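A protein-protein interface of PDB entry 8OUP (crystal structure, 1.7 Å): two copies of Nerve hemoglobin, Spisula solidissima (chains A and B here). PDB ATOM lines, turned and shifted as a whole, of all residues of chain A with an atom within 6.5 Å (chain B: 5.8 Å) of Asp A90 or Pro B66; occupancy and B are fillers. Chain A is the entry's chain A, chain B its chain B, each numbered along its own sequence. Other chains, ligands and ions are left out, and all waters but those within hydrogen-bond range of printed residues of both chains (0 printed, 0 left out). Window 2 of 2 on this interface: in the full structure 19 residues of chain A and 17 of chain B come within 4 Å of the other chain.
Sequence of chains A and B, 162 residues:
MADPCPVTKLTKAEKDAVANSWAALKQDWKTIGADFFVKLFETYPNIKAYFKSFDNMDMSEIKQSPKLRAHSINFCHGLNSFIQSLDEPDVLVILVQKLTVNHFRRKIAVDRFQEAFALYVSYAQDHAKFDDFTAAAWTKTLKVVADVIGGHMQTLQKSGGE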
ATOM      1  N   SER A  85     -30.804 -16.491 -25.167  1.00  0.00           N
ATOM      2  CA  SER A  85     -30.869 -16.867 -23.762  1.00  0.00           C
ATOM      3  C   SER A  85     -32.307 -17.001 -23.261  1.00  0.00           C
ATOM      4  O   SER A  85     -32.491 -17.084 -22.072  1.00  0.00           O
ATOM      5  CB  SER A  85     -30.084 -15.902 -22.919  1.00  0.00           C
ATOM      6  OG  SER A  85     -28.720 -15.912 -23.345  1.00  0.00           O
ATOM      7  N   GLU A  88     -32.770 -19.750 -20.854  1.00  0.00           N
ATOM      8  CA  GLU A  88     -31.940 -19.669 -19.652  1.00  0.00           C
ATOM      9  C   GLU A  88     -32.225 -18.357 -18.938  1.00  0.00           C
ATOM     10  O   GLU A  88     -31.479 -17.376 -18.989  1.00  0.00           O
ATOM     11  CB  GLU A  88     -30.448 -19.799 -19.984  1.00  0.00           C
ATOM     12  CG  GLU A  88     -30.145 -21.051 -20.765  1.00  0.00           C
ATOM     13  CD  GLU A  88     -28.697 -21.411 -21.066  1.00  0.00           C
ATOM     14  OE1 GLU A  88     -27.720 -20.682 -20.664  1.00  0.00           O
ATOM     15  OE2 GLU A  88     -28.544 -22.470 -21.717  1.00  0.00           O
ATOM     16  N   PRO A  89     -33.346 -18.273 -18.193  1.00  0.00           N
ATOM     17  CA  PRO A  89     -33.799 -17.007 -17.627  1.00  0.00           C
ATOM     18  C   PRO A  89     -32.839 -16.321 -16.661  1.00  0.00           C
ATOM     19  O   PRO A  89     -32.755 -15.096 -16.625  1.00  0.00           O
ATOM     20  CB  PRO A  89     -35.097 -17.372 -16.843  1.00  0.00           C
ATOM     21  CG  PRO A  89     -35.418 -18.773 -17.193  1.00  0.00           C
ATOM     22  CD  PRO A  89     -34.243 -19.401 -17.905  1.00  0.00           C
ATOM     23  N   ASP A  90     -32.018 -17.084 -15.936  1.00  0.00           N
ATOM     24  CA  ASP A  90     -31.066 -16.472 -15.029  1.00  0.00           C
ATOM     25  C   ASP A  90     -29.986 -15.739 -15.829  1.00  0.00           C
ATOM     26  O   ASP A  90     -29.513 -14.693 -15.404  1.00  0.00           O
ATOM     27  CB  ASP A  90     -30.410 -17.503 -14.117  1.00  0.00           C
ATOM     28  CG  ASP A  90     -31.301 -17.910 -12.956  1.00  0.00           C
ATOM     29  OD1 ASP A  90     -32.395 -17.332 -12.848  1.00  0.00           O
ATOM     30  OD2 ASP A  90     -30.897 -18.816 -12.188  1.00  0.00           O
ATOM     31  N   VAL A  91     -29.621 -16.353 -16.960  1.00  0.00           N
ATOM     32  CA  VAL A  91     -28.621 -15.759 -17.859  1.00  0.00           C
ATOM     33  C   VAL A  91     -29.204 -14.524 -18.547  1.00  0.00           C
ATOM     34  O   VAL A  91     -28.559 -13.488 -18.608  1.00  0.00           O
ATOM     35  CB  VAL A  91     -28.104 -16.772 -18.892  1.00  0.00           C
ATOM     36  CG1 VAL A  91     -27.148 -16.093 -19.875  1.00  0.00           C
ATOM     37  CG2 VAL A  91     -27.446 -17.989 -18.223  1.00  0.00           C
ATOM     38  N   LEU A  92     -30.424 -14.631 -19.067  1.00  0.00           N
ATOM     39  CA  LEU A  92     -31.088 -13.487 -19.685  1.00  0.00           C
ATOM     40  C   LEU A  92     -31.072 -12.291 -18.742  1.00  0.00           C
ATOM     41  O   LEU A  92     -30.743 -11.177 -19.132  1.00  0.00           O
ATOM     42  CB  LEU A  92     -32.514 -13.896 -20.051  1.00  0.00           C
ATOM     43  CG  LEU A  92     -33.397 -12.799 -20.646  1.00  0.00           C
ATOM     44  CD1 LEU A  92     -32.823 -12.329 -21.991  1.00  0.00           C
ATOM     45  CD2 LEU A  92     -34.835 -13.306 -20.815  1.00  0.00           C
ATOM     46  N   VAL A  93     -31.479 -12.509 -17.483  1.00  0.00           N
ATOM     47  CA  VAL A  93     -31.561 -11.444 -16.514  1.00  0.00           C
ATOM     48  C   VAL A  93     -30.207 -10.763 -16.330  1.00  0.00           C
ATOM     49  O   VAL A  93     -30.113  -9.523 -16.231  1.00  0.00           O
ATOM     50  CB  VAL A  93     -32.136 -11.963 -15.176  1.00  0.00           C
ATOM     51  CG1 VAL A  93     -31.888 -10.955 -14.066  1.00  0.00           C
ATOM     52  CG2 VAL A  93     -33.615 -12.305 -15.314  1.00  0.00           C
ATOM     53  N   ILE A  94     -29.129 -11.561 -16.264  1.00  0.00           N
ATOM     54  CA  ILE A  94     -27.817 -10.980 -16.078  1.00  0.00           C
ATOM     55  C   ILE A  94     -27.457 -10.092 -17.271  1.00  0.00           C
ATOM     56  O   ILE A  94     -26.973  -8.978 -17.045  1.00  0.00           O
ATOM     57  CB  ILE A  94     -26.764 -12.058 -15.796  1.00  0.00           C
ATOM     58  CG1 ILE A  94     -27.002 -12.631 -14.395  1.00  0.00           C
ATOM     59  CG2 ILE A  94     -25.367 -11.492 -15.917  1.00  0.00           C
ATOM     60  CD1 ILE A  94     -26.286 -13.909 -14.167  1.00  0.00           C
ATOM     61  N   LEU A  95     -27.649 -10.634 -18.476  1.00  0.00           N
ATOM     62  CA  LEU A  95     -27.304  -9.905 -19.706  1.00  0.00           C
ATOM     63  C   LEU A  95     -28.086  -8.580 -19.757  1.00  0.00           C
ATOM     64  O   LEU A  95     -27.540  -7.500 -20.072  1.00  0.00           O
ATOM     65  CB  LEU A  95     -27.622 -10.761 -20.926  1.00  0.00           C
ATOM     66  CG  LEU A  95     -26.791 -12.025 -21.156  1.00  0.00           C
ATOM     67  CD1 LEU A  95     -27.379 -12.873 -22.236  1.00  0.00           C
ATOM     68  CD2 LEU A  95     -25.334 -11.685 -21.491  1.00  0.00           C
ATOM     69  N   GLN B  64     -20.728 -23.715 -13.774  1.00  0.00           N
ATOM     70  CA  GLN B  64     -22.176 -23.776 -13.977  1.00  0.00           C
ATOM     71  C   GLN B  64     -22.902 -22.451 -13.765  1.00  0.00           C
ATOM     72  O   GLN B  64     -24.134 -22.362 -13.965  1.00  0.00           O
ATOM     73  CB  GLN B  64     -22.788 -24.749 -12.951  1.00  0.00           C
ATOM     74  CG  GLN B  64     -22.198 -26.138 -12.997  1.00  0.00           C
ATOM     75  CD  GLN B  64     -22.256 -26.749 -14.371  1.00  0.00           C
ATOM     76  OE1 GLN B  64     -21.276 -27.323 -14.851  1.00  0.00           O
ATOM     77  NE2 GLN B  64     -23.419 -26.639 -15.003  1.00  0.00           N
ATOM     78  N   SER B  65     -22.201 -21.422 -13.295  1.00  0.00           N
ATOM     79  CA  SER B  65     -22.846 -20.202 -12.858  1.00  0.00           C
ATOM     80  C   SER B  65     -23.432 -19.450 -14.055  1.00  0.00           C
ATOM     81  O   SER B  65     -22.874 -19.414 -15.157  1.00  0.00           O
ATOM     82  CB  SER B  65     -21.916 -19.342 -12.070  1.00  0.00           C
ATOM     83  OG  SER B  65     -20.966 -18.710 -12.910  1.00  0.00           O
ATOM     84  N   PRO B  66     -24.629 -18.874 -13.893  1.00  0.00           N
ATOM     85  CA  PRO B  66     -25.185 -18.023 -14.949  1.00  0.00           C
ATOM     86  C   PRO B  66     -24.297 -16.805 -15.211  1.00  0.00           C
ATOM     87  O   PRO B  66     -24.262 -16.312 -16.328  1.00  0.00           O
ATOM     88  CB  PRO B  66     -26.571 -17.603 -14.450  1.00  0.00           C
ATOM     89  CG  PRO B  66     -26.862 -18.485 -13.247  1.00  0.00           C
ATOM     90  CD  PRO B  66     -25.572 -19.108 -12.776  1.00  0.00           C
ATOM     91  N   LYS B  67     -23.518 -16.349 -14.225  1.00  0.00           N
ATOM     92  CA  LYS B  67     -22.656 -15.211 -14.446  1.00  0.00           C
ATOM     93  C   LYS B  67     -21.527 -15.599 -15.398  1.00  0.00           C
ATOM     94  O   LYS B  67     -21.167 -14.784 -16.256  1.00  0.00           O
ATOM     95  CB  LYS B  67     -22.070 -14.669 -13.143  1.00  0.00           C
ATOM     96  CG  LYS B  67     -23.122 -14.150 -12.161  1.00  0.00           C
ATOM     97  CD  LYS B  67     -22.743 -12.841 -11.543  1.00  0.00           C
ATOM     98  CE  LYS B  67     -23.854 -12.245 -10.700  1.00  0.00           C
ATOM     99  NZ  LYS B  67     -23.825 -10.770 -10.762  1.00  0.00           N
ATOM    100  N   LEU B  68     -21.017 -16.834 -15.287  1.00  0.00           N
ATOM    101  CA  LEU B  68     -19.943 -17.246 -16.168  1.00  0.00           C
ATOM    102  C   LEU B  68     -20.518 -17.386 -17.569  1.00  0.00           C
ATOM    103  O   LEU B  68     -19.892 -16.927 -18.537  1.00  0.00           O
ATOM    104  CB  LEU B  68     -19.308 -18.570 -15.762  1.00  0.00           C
ATOM    105  CG  LEU B  68     -18.095 -18.905 -16.632  1.00  0.00           C
ATOM    106  CD1 LEU B  68     -17.027 -17.865 -16.407  1.00  0.00           C
ATOM    107  CD2 LEU B  68     -17.605 -20.306 -16.349  1.00  0.00           C
ATOM    108  N   ARG B  69     -21.696 -18.032 -17.666  1.00  0.00           N
ATOM    109  CA  ARG B  69     -22.344 -18.259 -18.942  1.00  0.00           C
ATOM    110  C   ARG B  69     -22.621 -16.907 -19.620  1.00  0.00           C
ATOM    111  O   ARG B  69     -22.430 -16.761 -20.842  1.00  0.00           O
ATOM    112  CB  ARG B  69     -23.511 -19.209 -18.670  1.00  0.00           C
ATOM    113  CG  ARG B  69     -23.038 -20.636 -18.424  1.00  0.00           C
ATOM    114  CD  ARG B  69     -23.915 -21.478 -17.506  1.00  0.00           C
ATOM    115  NE  ARG B  69     -25.280 -21.424 -17.950  1.00  0.00           N
ATOM    116  CZ  ARG B  69     -26.341 -21.404 -17.155  1.00  0.00           C
ATOM    117  NH1 ARG B  69     -26.213 -21.281 -15.847  1.00  0.00           N
ATOM    118  NH2 ARG B  69     -27.537 -21.511 -17.694  1.00  0.00           N
ATOM    119  N   ALA B  70     -23.057 -15.909 -18.844  1.00  0.00           N
ATOM    120  CA  ALA B  70     -23.324 -14.599 -19.426  1.00  0.00           C
ATOM    121  C   ALA B  70     -22.019 -14.004 -19.975  1.00  0.00           C
ATOM    122  O   ALA B  70     -22.007 -13.467 -21.093  1.00  0.00           O
ATOM    123  CB  ALA B  70     -23.991 -13.709 -18.403  1.00  0.00           C
ATOM    124  N   HIS B  71     -20.929 -14.110 -19.213  1.00  0.00           N
ATOM    125  CA  HIS B  71     -19.692 -13.523 -19.722  1.00  0.00           C
ATOM    126  C   HIS B  71     -19.236 -14.243 -20.981  1.00  0.00           C
ATOM    127  O   HIS B  71     -18.663 -13.633 -21.868  1.00  0.00           O
ATOM    128  CB  HIS B  71     -18.563 -13.477 -18.704  1.00  0.00           C
ATOM    129  CG  HIS B  71     -17.414 -12.643 -19.183  1.00  0.00           C
ATOM    130  ND1 HIS B  71     -16.267 -13.155 -19.737  1.00  0.00           N
ATOM    131  CD2 HIS B  71     -17.302 -11.292 -19.229  1.00  0.00           C
ATOM    132  CE1 HIS B  71     -15.476 -12.145 -20.095  1.00  0.00           C
ATOM    133  NE2 HIS B  71     -16.070 -10.988 -19.777  1.00  0.00           N
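The guanidinium group of Arg B69 is in salt-bridge range of the side-chain carboxylate of Glu A88 (3.1 Å).
O of Gln B64 is in hydrogen-bond range of NH1 of Arg B69 (3.0 Å).
Among the printed residues, merely in contact across the chains: Asp A90 with Pro B66, Val A91 with Pro B66, Val A91 with Arg B69, Ile A94 with Pro B66, Ile A94 with Lys B67, Ile A94 with Ala B70 and Leu A95 with Ala B70.
Asp A90 touches just one residue of chain B: Pro B66 (3.8 Å). Pro B66 touches just these residues of chain A: Asp A90 (3.8 Å), Val A91 (3.9 Å) and Ile A94 (3.7 Å). Printed residues of chain A within 4 Å of Arg B69: Glu A88 and Val A91. Printed residues of chain B within 4 Å of Glu A88: Arg B69. Printed residues of chain B within 4 Å of Leu A95: Ala B70.
Of the 9 printed residues of chain A, 5 touch a printed residue of chain B. Printed residues of chain A that touch a printed residue of chain B: Glu A88, Asp A90, Val A91, Ile A94 and Leu A95. Hydrophobic or aromatic side chains of chain A within 4 Å of the printed part of chain B: Val A91, Ile A94 and Leu A95. Printed residues of chain B that touch a printed residue of chain A: Pro B66, Lys B67, Arg B69 and Ala B70. Along chain B the printed residues that touch a printed residue of chain A span positions 66 to 70. Among the printed residues, 8 pairs touch across the chains.
No position is printed for both chains. Of the 8 pairs that touch across the chains among the printed residues, none has its exchanged pair printed and touching as well.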
